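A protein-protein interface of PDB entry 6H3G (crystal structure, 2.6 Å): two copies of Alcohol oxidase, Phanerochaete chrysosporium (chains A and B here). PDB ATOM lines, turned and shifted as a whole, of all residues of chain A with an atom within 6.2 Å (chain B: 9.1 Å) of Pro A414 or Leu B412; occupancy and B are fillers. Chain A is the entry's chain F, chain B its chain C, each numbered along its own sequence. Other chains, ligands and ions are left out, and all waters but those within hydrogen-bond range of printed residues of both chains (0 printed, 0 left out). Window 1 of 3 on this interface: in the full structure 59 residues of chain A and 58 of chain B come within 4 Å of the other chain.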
ATOM      1  N   ARG A 321     -28.510  32.452   1.622  1.00  0.00           N
ATOM      2  CA  ARG A 321     -27.178  33.039   1.701  1.00  0.00           C
ATOM      3  C   ARG A 321     -27.311  34.556   1.757  1.00  0.00           C
ATOM      4  O   ARG A 321     -28.185  35.108   1.099  1.00  0.00           O
ATOM      5  CB  ARG A 321     -26.352  32.653   0.471  1.00  0.00           C
ATOM      6  CG  ARG A 321     -25.912  31.197   0.449  1.00  0.00           C
ATOM      7  CD  ARG A 321     -25.348  30.840  -0.907  1.00  0.00           C
ATOM      8  NE  ARG A 321     -24.228  29.909  -0.838  1.00  0.00           N
ATOM      9  CZ  ARG A 321     -23.014  30.223  -0.400  1.00  0.00           C
ATOM     10  NH1 ARG A 321     -22.802  31.392   0.178  1.00  0.00           N
ATOM     11  NH2 ARG A 321     -22.019  29.367  -0.530  1.00  0.00           N
ATOM     12  N   ARG A 334     -19.309  27.818  13.795  1.00  0.00           N
ATOM     13  CA  ARG A 334     -18.202  27.095  13.168  1.00  0.00           C
ATOM     14  C   ARG A 334     -17.122  26.799  14.222  1.00  0.00           C
ATOM     15  O   ARG A 334     -16.468  25.759  14.177  1.00  0.00           O
ATOM     16  CB  ARG A 334     -17.650  27.868  11.961  1.00  0.00           C
ATOM     17  CG  ARG A 334     -18.412  27.619  10.665  1.00  0.00           C
ATOM     18  CD  ARG A 334     -18.005  28.535   9.526  1.00  0.00           C
ATOM     19  NE  ARG A 334     -18.798  28.305   8.322  1.00  0.00           N
ATOM     20  CZ  ARG A 334     -19.434  29.246   7.620  1.00  0.00           C
ATOM     21  NH1 ARG A 334     -19.348  30.521   7.962  1.00  0.00           N
ATOM     22  NH2 ARG A 334     -20.153  28.906   6.565  1.00  0.00           N
ATOM     23  N   HIS A 410     -22.785  22.802   9.722  1.00  0.00           N
ATOM     24  CA  HIS A 410     -21.942  23.708   8.897  1.00  0.00           C
ATOM     25  C   HIS A 410     -20.890  22.910   8.113  1.00  0.00           C
ATOM     26  O   HIS A 410     -20.365  23.385   7.076  1.00  0.00           O
ATOM     27  CB  HIS A 410     -21.302  24.801   9.763  1.00  0.00           C
ATOM     28  CG  HIS A 410     -22.247  25.890  10.148  1.00  0.00           C
ATOM     29  ND1 HIS A 410     -23.264  25.696  11.067  1.00  0.00           N
ATOM     30  CD2 HIS A 410     -22.341  27.176   9.742  1.00  0.00           C
ATOM     31  CE1 HIS A 410     -23.945  26.818  11.206  1.00  0.00           C
ATOM     32  NE2 HIS A 410     -23.400  27.743  10.408  1.00  0.00           N
ATOM     33  N   LEU A 412     -21.855  20.577   6.417  1.00  0.00           N
ATOM     34  CA  LEU A 412     -22.575  20.300   5.145  1.00  0.00           C
ATOM     35  C   LEU A 412     -22.904  21.590   4.377  1.00  0.00           C
ATOM     36  O   LEU A 412     -23.544  21.532   3.317  1.00  0.00           O
ATOM     37  CB  LEU A 412     -23.873  19.550   5.454  1.00  0.00           C
ATOM     38  CG  LEU A 412     -23.891  18.064   5.118  1.00  0.00           C
ATOM     39  CD1 LEU A 412     -23.738  17.837   3.623  1.00  0.00           C
ATOM     40  CD2 LEU A 412     -22.828  17.320   5.906  1.00  0.00           C
ATOM     41  N   LEU A 413     -22.482  22.739   4.915  1.00  0.00           N
ATOM     42  CA  LEU A 413     -22.737  24.042   4.319  1.00  0.00           C
ATOM     43  C   LEU A 413     -21.460  24.577   3.702  1.00  0.00           C
ATOM     44  O   LEU A 413     -20.403  24.510   4.326  1.00  0.00           O
ATOM     45  CB  LEU A 413     -23.175  25.046   5.386  1.00  0.00           C
ATOM     46  CG  LEU A 413     -24.501  24.774   6.079  1.00  0.00           C
ATOM     47  CD1 LEU A 413     -24.662  25.725   7.251  1.00  0.00           C
ATOM     48  CD2 LEU A 413     -25.668  24.909   5.109  1.00  0.00           C
ATOM     49  N   PRO A 414     -21.553  25.205   2.512  1.00  0.00           N
ATOM     50  CA  PRO A 414     -20.443  25.974   1.952  1.00  0.00           C
ATOM     51  C   PRO A 414     -19.969  27.072   2.898  1.00  0.00           C
ATOM     52  O   PRO A 414     -20.625  27.362   3.892  1.00  0.00           O
ATOM     53  CB  PRO A 414     -21.044  26.627   0.698  1.00  0.00           C
ATOM     54  CG  PRO A 414     -22.200  25.725   0.321  1.00  0.00           C
ATOM     55  CD  PRO A 414     -22.734  25.192   1.633  1.00  0.00           C
ATOM     56  N   PRO A 415     -18.848  27.758   2.600  1.00  0.00           N
ATOM     57  CA  PRO A 415     -18.461  28.927   3.378  1.00  0.00           C
ATOM     58  C   PRO A 415     -19.460  30.057   3.104  1.00  0.00           C
ATOM     59  O   PRO A 415     -20.294  29.936   2.200  1.00  0.00           O
ATOM     60  CB  PRO A 415     -17.071  29.266   2.827  1.00  0.00           C
ATOM     61  CG  PRO A 415     -17.159  28.813   1.390  1.00  0.00           C
ATOM     62  CD  PRO A 415     -17.940  27.514   1.467  1.00  0.00           C
ATOM     63  N   GLY A 416     -19.333  31.136   3.876  1.00  0.00           N
ATOM     64  CA  GLY A 416     -20.163  32.316   3.738  1.00  0.00           C
ATOM     65  C   GLY A 416     -21.102  32.471   4.920  1.00  0.00           C
ATOM     66  O   GLY A 416     -20.986  31.751   5.923  1.00  0.00           O
ATOM     67  N   TYR A 418     -25.272  33.094   6.301  1.00  0.00           N
ATOM     68  CA  TYR A 418     -26.535  32.473   6.077  1.00  0.00           C
ATOM     69  C   TYR A 418     -27.571  33.106   7.006  1.00  0.00           C
ATOM     70  O   TYR A 418     -27.220  33.807   7.953  1.00  0.00           O
ATOM     71  CB  TYR A 418     -26.427  30.966   6.328  1.00  0.00           C
ATOM     72  CG  TYR A 418     -25.481  30.239   5.400  1.00  0.00           C
ATOM     73  CD1 TYR A 418     -25.793  30.059   4.057  1.00  0.00           C
ATOM     74  CD2 TYR A 418     -24.274  29.727   5.853  1.00  0.00           C
ATOM     75  CE1 TYR A 418     -24.940  29.386   3.198  1.00  0.00           C
ATOM     76  CE2 TYR A 418     -23.406  29.057   5.005  1.00  0.00           C
ATOM     77  CZ  TYR A 418     -23.740  28.886   3.671  1.00  0.00           C
ATOM     78  OH  TYR A 418     -22.894  28.233   2.820  1.00  0.00           O
ATOM     79  N   LEU A 482     -29.490  28.628  -0.848  1.00  0.00           N
ATOM     80  CA  LEU A 482     -28.525  27.555  -0.849  1.00  0.00           C
ATOM     81  C   LEU A 482     -29.149  26.388  -1.605  1.00  0.00           C
ATOM     82  O   LEU A 482     -29.857  25.572  -1.015  1.00  0.00           O
ATOM     83  CB  LEU A 482     -28.134  27.143   0.573  1.00  0.00           C
ATOM     84  CG  LEU A 482     -27.107  26.006   0.648  1.00  0.00           C
ATOM     85  CD1 LEU A 482     -25.770  26.431   0.060  1.00  0.00           C
ATOM     86  CD2 LEU A 482     -26.906  25.525   2.070  1.00  0.00           C
ATOM     87  N   THR A 483     -28.868  26.333  -2.912  1.00  0.00           N
ATOM     88  CA  THR A 483     -29.403  25.316  -3.827  1.00  0.00           C
ATOM     89  C   THR A 483     -29.406  23.940  -3.137  1.00  0.00           C
ATOM     90  O   THR A 483     -30.433  23.290  -3.075  1.00  0.00           O
ATOM     91  CB  THR A 483     -28.649  25.366  -5.166  1.00  0.00           C
ATOM     92  OG1 THR A 483     -28.791  26.675  -5.724  1.00  0.00           O
ATOM     93  CG2 THR A 483     -29.146  24.357  -6.179  1.00  0.00           C
ATOM     94  N   SER A 484     -28.268  23.536  -2.562  1.00  0.00           N
ATOM     95  CA  SER A 484     -28.078  22.181  -2.017  1.00  0.00           C
ATOM     96  C   SER A 484     -29.169  21.798  -1.001  1.00  0.00           C
ATOM     97  O   SER A 484     -29.494  20.623  -0.888  1.00  0.00           O
ATOM     98  CB  SER A 484     -26.679  22.006  -1.428  1.00  0.00           C
ATOM     99  OG  SER A 484     -26.325  23.055  -0.528  1.00  0.00           O
ATOM    100  N   HIS A 485     -29.715  22.780  -0.266  1.00  0.00           N
ATOM    101  CA  HIS A 485     -30.595  22.545   0.912  1.00  0.00           C
ATOM    102  C   HIS A 485     -32.042  22.963   0.604  1.00  0.00           C
ATOM    103  O   HIS A 485     -32.859  23.156   1.534  1.00  0.00           O
ATOM    104  CB  HIS A 485     -30.037  23.279   2.146  1.00  0.00           C
ATOM    105  CG  HIS A 485     -28.832  22.634   2.750  1.00  0.00           C
ATOM    106  ND1 HIS A 485     -27.719  22.292   2.001  1.00  0.00           N
ATOM    107  CD2 HIS A 485     -28.552  22.277   4.023  1.00  0.00           C
ATOM    108  CE1 HIS A 485     -26.814  21.745   2.787  1.00  0.00           C
ATOM    109  NE2 HIS A 485     -27.297  21.726   4.035  1.00  0.00           N
ATOM    110  N   ASP A 499     -28.282  30.579  -6.577  1.00  0.00           N
ATOM    111  CA  ASP A 499     -27.317  30.476  -5.490  1.00  0.00           C
ATOM    112  C   ASP A 499     -26.520  31.787  -5.428  1.00  0.00           C
ATOM    113  O   ASP A 499     -26.964  32.799  -5.941  1.00  0.00           O
ATOM    114  CB  ASP A 499     -26.470  29.208  -5.650  1.00  0.00           C
ATOM    115  CG  ASP A 499     -25.973  28.614  -4.339  1.00  0.00           C
ATOM    116  OD1 ASP A 499     -25.240  29.336  -3.623  1.00  0.00           O
ATOM    117  OD2 ASP A 499     -26.312  27.433  -4.044  1.00  0.00           O
ATOM    118  N   ILE A 500     -25.359  31.757  -4.763  1.00  0.00           N
ATOM    119  CA  ILE A 500     -24.549  32.948  -4.474  1.00  0.00           C
ATOM    120  C   ILE A 500     -24.106  33.620  -5.782  1.00  0.00           C
ATOM    121  O   ILE A 500     -23.762  32.945  -6.749  1.00  0.00           O
ATOM    122  CB  ILE A 500     -23.342  32.583  -3.584  1.00  0.00           C
ATOM    123  CG1 ILE A 500     -22.571  33.828  -3.149  1.00  0.00           C
ATOM    124  CG2 ILE A 500     -22.426  31.571  -4.260  1.00  0.00           C
ATOM    125  CD1 ILE A 500     -21.703  33.598  -1.946  1.00  0.00           C
ATOM    126  N   TRP A 522     -23.021  23.464 -11.112  1.00  0.00           N
ATOM    127  CA  TRP A 522     -23.666  22.937  -9.908  1.00  0.00           C
ATOM    128  C   TRP A 522     -24.649  23.954  -9.319  1.00  0.00           C
ATOM    129  O   TRP A 522     -25.482  23.584  -8.477  1.00  0.00           O
ATOM    130  CB  TRP A 522     -22.622  22.545  -8.859  1.00  0.00           C
ATOM    131  CG  TRP A 522     -21.551  21.621  -9.344  1.00  0.00           C
ATOM    132  CD1 TRP A 522     -20.227  21.918  -9.465  1.00  0.00           C
ATOM    133  CD2 TRP A 522     -21.694  20.241  -9.731  1.00  0.00           C
ATOM    134  NE1 TRP A 522     -19.535  20.818  -9.895  1.00  0.00           N
ATOM    135  CE2 TRP A 522     -20.407  19.776 -10.067  1.00  0.00           C
ATOM    136  CE3 TRP A 522     -22.769  19.349  -9.817  1.00  0.00           C
ATOM    137  CZ2 TRP A 522     -20.176  18.469 -10.495  1.00  0.00           C
ATOM    138  CZ3 TRP A 522     -22.540  18.059 -10.241  1.00  0.00           C
ATOM    139  CH2 TRP A 522     -21.261  17.626 -10.576  1.00  0.00           C
ATOM    140  N   HIS A 523     -24.530  25.222  -9.728  1.00  0.00           N
ATOM    141  CA  HIS A 523     -25.375  26.266  -9.204  1.00  0.00           C
ATOM    142  C   HIS A 523     -25.645  27.309 -10.284  1.00  0.00           C
ATOM    143  O   HIS A 523     -24.758  27.627 -11.044  1.00  0.00           O
ATOM    144  CB  HIS A 523     -24.721  26.891  -7.970  1.00  0.00           C
ATOM    145  CG  HIS A 523     -23.584  27.799  -8.285  1.00  0.00           C
ATOM    146  ND1 HIS A 523     -23.695  29.172  -8.204  1.00  0.00           N
ATOM    147  CD2 HIS A 523     -22.314  27.542  -8.663  1.00  0.00           C
ATOM    148  CE1 HIS A 523     -22.541  29.727  -8.518  1.00  0.00           C
ATOM    149  NE2 HIS A 523     -21.674  28.746  -8.801  1.00  0.00           N
ATOM    150  N   ILE B 319     -17.621  14.129  -7.361  1.00  0.00           N
ATOM    151  CA  ILE B 319     -16.838  14.630  -6.236  1.00  0.00           C
ATOM    152  C   ILE B 319     -17.123  13.770  -5.002  1.00  0.00           C
ATOM    153  O   ILE B 319     -18.252  13.329  -4.766  1.00  0.00           O
ATOM    154  CB  ILE B 319     -17.085  16.131  -5.991  1.00  0.00           C
ATOM    155  CG1 ILE B 319     -16.620  16.971  -7.183  1.00  0.00           C
ATOM    156  CG2 ILE B 319     -16.410  16.590  -4.712  1.00  0.00           C
ATOM    157  CD1 ILE B 319     -17.111  18.398  -7.171  1.00  0.00           C
ATOM    158  N   ARG B 321     -15.755  13.109  -0.773  1.00  0.00           N
ATOM    159  CA  ARG B 321     -15.127  13.623   0.419  1.00  0.00           C
ATOM    160  C   ARG B 321     -14.081  12.618   0.887  1.00  0.00           C
ATOM    161  O   ARG B 321     -14.282  11.411   0.788  1.00  0.00           O
ATOM    162  CB  ARG B 321     -16.177  13.864   1.506  1.00  0.00           C
ATOM    163  CG  ARG B 321     -17.067  15.070   1.239  1.00  0.00           C
ATOM    164  CD  ARG B 321     -18.316  15.024   2.088  1.00  0.00           C
ATOM    165  NE  ARG B 321     -18.793  16.339   2.498  1.00  0.00           N
ATOM    166  CZ  ARG B 321     -18.215  17.087   3.426  1.00  0.00           C
ATOM    167  NH1 ARG B 321     -17.058  16.717   3.949  1.00  0.00           N
ATOM    168  NH2 ARG B 321     -18.777  18.215   3.808  1.00  0.00           N
ATOM    169  N   ARG B 334      -8.359  27.213  -1.979  1.00  0.00           N
ATOM    170  CA  ARG B 334      -9.232  28.102  -1.175  1.00  0.00           C
ATOM    171  C   ARG B 334      -8.561  29.458  -0.927  1.00  0.00           C
ATOM    172  O   ARG B 334      -9.236  30.442  -0.629  1.00  0.00           O
ATOM    173  CB  ARG B 334      -9.602  27.467   0.169  1.00  0.00           C
ATOM    174  CG  ARG B 334     -10.788  26.516   0.095  1.00  0.00           C
ATOM    175  CD  ARG B 334     -11.158  25.957   1.454  1.00  0.00           C
ATOM    176  NE  ARG B 334     -12.214  24.959   1.354  1.00  0.00           N
ATOM    177  CZ  ARG B 334     -12.039  23.657   1.538  1.00  0.00           C
ATOM    178  NH1 ARG B 334     -10.867  23.207   1.960  1.00  0.00           N
ATOM    179  NH2 ARG B 334     -13.025  22.812   1.294  1.00  0.00           N
ATOM    180  N   ALA B 406     -10.969  18.994  -5.104  1.00  0.00           N
ATOM    181  CA  ALA B 406     -12.188  19.235  -5.869  1.00  0.00           C
ATOM    182  C   ALA B 406     -11.896  20.230  -6.996  1.00  0.00           C
ATOM    183  O   ALA B 406     -11.382  21.321  -6.737  1.00  0.00           O
ATOM    184  CB  ALA B 406     -13.271  19.762  -4.960  1.00  0.00           C
ATOM    185  N   ALA B 408     -13.860  22.351  -8.565  1.00  0.00           N
ATOM    186  CA  ALA B 408     -15.173  22.985  -8.443  1.00  0.00           C
ATOM    187  C   ALA B 408     -15.060  24.265  -7.607  1.00  0.00           C
ATOM    188  O   ALA B 408     -14.094  24.459  -6.869  1.00  0.00           O
ATOM    189  CB  ALA B 408     -16.157  22.016  -7.829  1.00  0.00           C
ATOM    190  N   ASP B 409     -16.067  25.131  -7.741  1.00  0.00           N
ATOM    191  CA  ASP B 409     -16.168  26.367  -6.979  1.00  0.00           C
ATOM    192  C   ASP B 409     -16.316  26.009  -5.490  1.00  0.00           C
ATOM    193  O   ASP B 409     -17.365  25.579  -5.071  1.00  0.00           O
ATOM    194  CB  ASP B 409     -17.324  27.208  -7.541  1.00  0.00           C
ATOM    195  CG  ASP B 409     -17.311  28.681  -7.160  1.00  0.00           C
ATOM    196  OD1 ASP B 409     -16.763  29.010  -6.088  1.00  0.00           O
ATOM    197  OD2 ASP B 409     -17.861  29.490  -7.941  1.00  0.00           O
ATOM    198  N   HIS B 410     -15.230  26.143  -4.718  1.00  0.00           N
ATOM    199  CA  HIS B 410     -15.181  25.894  -3.240  1.00  0.00           C
ATOM    200  C   HIS B 410     -16.093  26.847  -2.447  1.00  0.00           C
ATOM    201  O   HIS B 410     -16.468  26.572  -1.318  1.00  0.00           O
ATOM    202  CB  HIS B 410     -13.749  26.038  -2.711  1.00  0.00           C
ATOM    203  CG  HIS B 410     -12.867  24.874  -3.003  1.00  0.00           C
ATOM    204  ND1 HIS B 410     -12.140  24.777  -4.171  1.00  0.00           N
ATOM    205  CD2 HIS B 410     -12.572  23.779  -2.269  1.00  0.00           C
ATOM    206  CE1 HIS B 410     -11.448  23.657  -4.155  1.00  0.00           C
ATOM    207  NE2 HIS B 410     -11.694  23.025  -2.996  1.00  0.00           N
ATOM    208  N   THR B 411     -16.387  28.001  -3.038  1.00  0.00           N
ATOM    209  CA  THR B 411     -17.467  28.896  -2.634  1.00  0.00           C
ATOM    210  C   THR B 411     -18.831  28.164  -2.637  1.00  0.00           C
ATOM    211  O   THR B 411     -19.766  28.676  -2.036  1.00  0.00           O
ATOM    212  CB  THR B 411     -17.392  30.156  -3.515  1.00  0.00           C
ATOM    213  OG1 THR B 411     -16.832  31.215  -2.739  1.00  0.00           O
ATOM    214  CG2 THR B 411     -18.715  30.584  -4.107  1.00  0.00           C
ATOM    215  N   LEU B 412     -18.947  26.991  -3.293  1.00  0.00           N
ATOM    216  CA  LEU B 412     -20.195  26.159  -3.375  1.00  0.00           C
ATOM    217  C   LEU B 412     -19.990  24.747  -2.805  1.00  0.00           C
ATOM    218  O   LEU B 412     -20.858  23.903  -2.981  1.00  0.00           O
ATOM    219  CB  LEU B 412     -20.629  26.022  -4.843  1.00  0.00           C
ATOM    220  CG  LEU B 412     -21.922  26.721  -5.273  1.00  0.00           C
ATOM    221  CD1 LEU B 412     -23.124  26.247  -4.470  1.00  0.00           C
ATOM    222  CD2 LEU B 412     -21.783  28.230  -5.191  1.00  0.00           C
ATOM    223  N   LEU B 413     -18.837  24.483  -2.180  1.00  0.00           N
ATOM    224  CA  LEU B 413     -18.529  23.196  -1.534  1.00  0.00           C
ATOM    225  C   LEU B 413     -18.382  23.388  -0.028  1.00  0.00           C
ATOM    226  O   LEU B 413     -17.658  24.282   0.410  1.00  0.00           O
ATOM    227  CB  LEU B 413     -17.184  22.649  -2.007  1.00  0.00           C
ATOM    228  CG  LEU B 413     -17.017  22.297  -3.475  1.00  0.00           C
ATOM    229  CD1 LEU B 413     -15.539  22.064  -3.747  1.00  0.00           C
ATOM    230  CD2 LEU B 413     -17.824  21.063  -3.836  1.00  0.00           C
ATOM    231  N   PRO B 414     -18.948  22.479   0.797  1.00  0.00           N
ATOM    232  CA  PRO B 414     -18.661  22.453   2.226  1.00  0.00           C
ATOM    233  C   PRO B 414     -17.173  22.413   2.550  1.00  0.00           C
ATOM    234  O   PRO B 414     -16.349  22.105   1.685  1.00  0.00           O
ATOM    235  CB  PRO B 414     -19.284  21.141   2.724  1.00  0.00           C
ATOM    236  CG  PRO B 414     -20.324  20.775   1.688  1.00  0.00           C
ATOM    237  CD  PRO B 414     -19.894  21.431   0.393  1.00  0.00           C
ATOM    238  N   PRO B 415     -16.802  22.665   3.826  1.00  0.00           N
ATOM    239  CA  PRO B 415     -15.404  22.614   4.247  1.00  0.00           C
ATOM    240  C   PRO B 415     -14.929  21.157   4.265  1.00  0.00           C
ATOM    241  O   PRO B 415     -15.764  20.230   4.218  1.00  0.00           O
ATOM    242  CB  PRO B 415     -15.443  23.186   5.666  1.00  0.00           C
ATOM    243  CG  PRO B 415     -16.808  22.755   6.163  1.00  0.00           C
ATOM    244  CD  PRO B 415     -17.709  22.925   4.955  1.00  0.00           C
ATOM    245  N   GLY B 416     -13.606  20.986   4.335  1.00  0.00           N
ATOM    246  CA  GLY B 416     -12.973  19.682   4.341  1.00  0.00           C
ATOM    247  C   GLY B 416     -12.241  19.396   3.041  1.00  0.00           C
ATOM    248  O   GLY B 416     -12.083  20.275   2.173  1.00  0.00           O
ATOM    249  N   TYR B 418     -11.392  16.820  -0.404  1.00  0.00           N
ATOM    250  CA  TYR B 418     -12.120  16.186  -1.491  1.00  0.00           C
ATOM    251  C   TYR B 418     -11.156  15.521  -2.485  1.00  0.00           C
ATOM    252  O   TYR B 418      -9.977  15.875  -2.572  1.00  0.00           O
ATOM    253  CB  TYR B 418     -12.960  17.230  -2.234  1.00  0.00           C
ATOM    254  CG  TYR B 418     -14.030  17.928  -1.428  1.00  0.00           C
ATOM    255  CD1 TYR B 418     -15.225  17.304  -1.117  1.00  0.00           C
ATOM    256  CD2 TYR B 418     -13.873  19.241  -1.030  1.00  0.00           C
ATOM    257  CE1 TYR B 418     -16.220  17.950  -0.404  1.00  0.00           C
ATOM    258  CE2 TYR B 418     -14.858  19.905  -0.322  1.00  0.00           C
ATOM    259  CZ  TYR B 418     -16.038  19.260  -0.002  1.00  0.00           C
ATOM    260  OH  TYR B 418     -17.005  19.920   0.704  1.00  0.00           O
ATOM    261  N   LEU B 482     -20.187  13.625  -1.954  1.00  0.00           N
ATOM    262  CA  LEU B 482     -20.753  14.945  -1.709  1.00  0.00           C
ATOM    263  C   LEU B 482     -22.157  15.036  -2.340  1.00  0.00           C
ATOM    264  O   LEU B 482     -22.318  15.486  -3.487  1.00  0.00           O
ATOM    265  CB  LEU B 482     -19.814  16.013  -2.276  1.00  0.00           C
ATOM    266  CG  LEU B 482     -20.292  17.449  -2.069  1.00  0.00           C
ATOM    267  CD1 LEU B 482     -20.341  17.786  -0.587  1.00  0.00           C
ATOM    268  CD2 LEU B 482     -19.423  18.443  -2.821  1.00  0.00           C
ATOM    269  N   SER B 484     -24.639  16.962  -2.476  1.00  0.00           N
ATOM    270  CA  SER B 484     -25.102  18.158  -3.197  1.00  0.00           C
ATOM    271  C   SER B 484     -24.810  18.057  -4.704  1.00  0.00           C
ATOM    272  O   SER B 484     -25.582  18.554  -5.507  1.00  0.00           O
ATOM    273  CB  SER B 484     -24.518  19.433  -2.596  1.00  0.00           C
ATOM    274  OG  SER B 484     -23.093  19.405  -2.530  1.00  0.00           O
ATOM    275  N   HIS B 485     -23.694  17.408  -5.066  1.00  0.00           N
ATOM    276  CA  HIS B 485     -23.128  17.429  -6.418  1.00  0.00           C
ATOM    277  C   HIS B 485     -23.269  16.065  -7.092  1.00  0.00           C
ATOM    278  O   HIS B 485     -22.576  15.772  -8.078  1.00  0.00           O
ATOM    279  CB  HIS B 485     -21.638  17.800  -6.364  1.00  0.00           C
ATOM    280  CG  HIS B 485     -21.381  19.222  -6.019  1.00  0.00           C
ATOM    281  ND1 HIS B 485     -21.892  19.804  -4.880  1.00  0.00           N
ATOM    282  CD2 HIS B 485     -20.653  20.166  -6.651  1.00  0.00           C
ATOM    283  CE1 HIS B 485     -21.518  21.063  -4.841  1.00  0.00           C
ATOM    284  NE2 HIS B 485     -20.744  21.310  -5.919  1.00  0.00           N
ATOM    285  N   TYR B 509     -14.521  20.901  12.327  1.00  0.00           N
ATOM    286  CA  TYR B 509     -14.934  21.953  13.230  1.00  0.00           C
ATOM    287  C   TYR B 509     -15.006  21.418  14.656  1.00  0.00           C
ATOM    288  O   TYR B 509     -16.099  21.199  15.175  1.00  0.00           O
ATOM    289  CB  TYR B 509     -16.309  22.482  12.825  1.00  0.00           C
ATOM    290  CG  TYR B 509     -16.368  23.293  11.557  1.00  0.00           C
ATOM    291  CD1 TYR B 509     -15.397  24.231  11.247  1.00  0.00           C
ATOM    292  CD2 TYR B 509     -17.455  23.170  10.701  1.00  0.00           C
ATOM    293  CE1 TYR B 509     -15.484  24.994  10.094  1.00  0.00           C
ATOM    294  CE2 TYR B 509     -17.560  23.930   9.547  1.00  0.00           C
ATOM    295  CZ  TYR B 509     -16.570  24.843   9.247  1.00  0.00           C
ATOM    296  OH  TYR B 509     -16.673  25.580   8.111  1.00  0.00           O
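Leu A412 touches Pro B414, and with the chains exchanged Pro A414 touches Leu B412. Leu A413 touches Pro B414, and with the chains exchanged Pro A414 touches Leu B413. Pro A414 touches its own counterpart, Pro B414. Ser A484 touches its own counterpart, Ser B484. Positions printed for both chains: 321, 334, 410, 412, 413, 414, 415, 416, 418, 482, 484 and 485. Of the 20 pairs that touch across the chains among the printed residues, 10 have their exchanged pair printed and touching as well.
Pro B415 touches His A410. Tyr B509 touches His A410. Pro B414 touches Leu A412 (CG to O, 3.7 Å). Leu A413 touches Pro B414 (O to CA, 3.4 Å). CA of Pro A414 touches O of Leu B413, at 3.6 Å. O of His B410 touches CD of Pro A415 (3.3 Å). Ser B484 touches Ser A484. Asp A499 touches Leu B412. CG2 of Ile A500 touches CG2 of Thr B411, at 3.8 Å. Asp B409 touches His A523.
Hydrophobic or aromatic side chains of chain B within 4 Å of the printed part of chain A: Leu B412, Pro B414, Pro B415, His B485 and Tyr B509. Among the printed residues, 20 pairs touch across the chains.
The backbone carbonyl oxygen (O) of Pro B414 lies within hydrogen-bond range of the guanidinium group (NH2) of Arg B334. The side-chain carboxylate (OD1) of Asp B409 lies close to the backbone NH (N) of Thr B411, at 3.2 Å. O of Pro B414 is in hydrogen-bond range of OH of Tyr B418 (2.5 Å). A ring nitrogen (ND1) of His B485 lies within hydrogen-bond range of the side-chain hydroxyl (OG) of Ser B484 (2.7 Å). The backbone carbonyl oxygen (O) of Pro A414 lies within hydrogen-bond range of the guanidinium group (NH2) of Arg A334 (3.1 Å). The side-chain hydroxyl (OG) of Ser A484 sits at hydrogen-bond distance from a ring nitrogen (ND1) of His A485 (3.0 Å).
Of the printed residues of chain B, His A410 touches Pro B415 (3.4 Å) and Tyr B509 (3.8 Å). Pro A414 touches just these residues of chain B: Thr B411, Leu B412, Leu B413 and Pro B414. Of chain B, only His B410 (3.3 Å) and Leu B413 (3.4 Å) come within 4 Å of Pro A415. Of the printed residues of chain B, Trp A522 touches His B485 (3.1 Å). Of the printed residues of chain B, His A523 touches Asp B409 (3.98 Å) and Leu B412 (3.5 Å). Printed residues of chain A within 4 Å of Asp B409: His A523 (3.98 Å). Leu B412 touches four residues of chain A. Printed residues of chain A within 4 Å of Ser B484: Ser A484. The nearest residue of chain A that does not touch Leu B412 is Arg A321 (4.7 Å). The nearest printed residue of chain B that does not touch Arg A321 is Leu B412 (4.7 Å).
The backbone carbonyl oxygen of Thr B411 is in hydrogen-bond range of the guanidinium group of Arg A321 (2.8 Å). OH of Tyr B509 lies within hydrogen-bond range of NE of Arg A334, at 3.5 Å.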
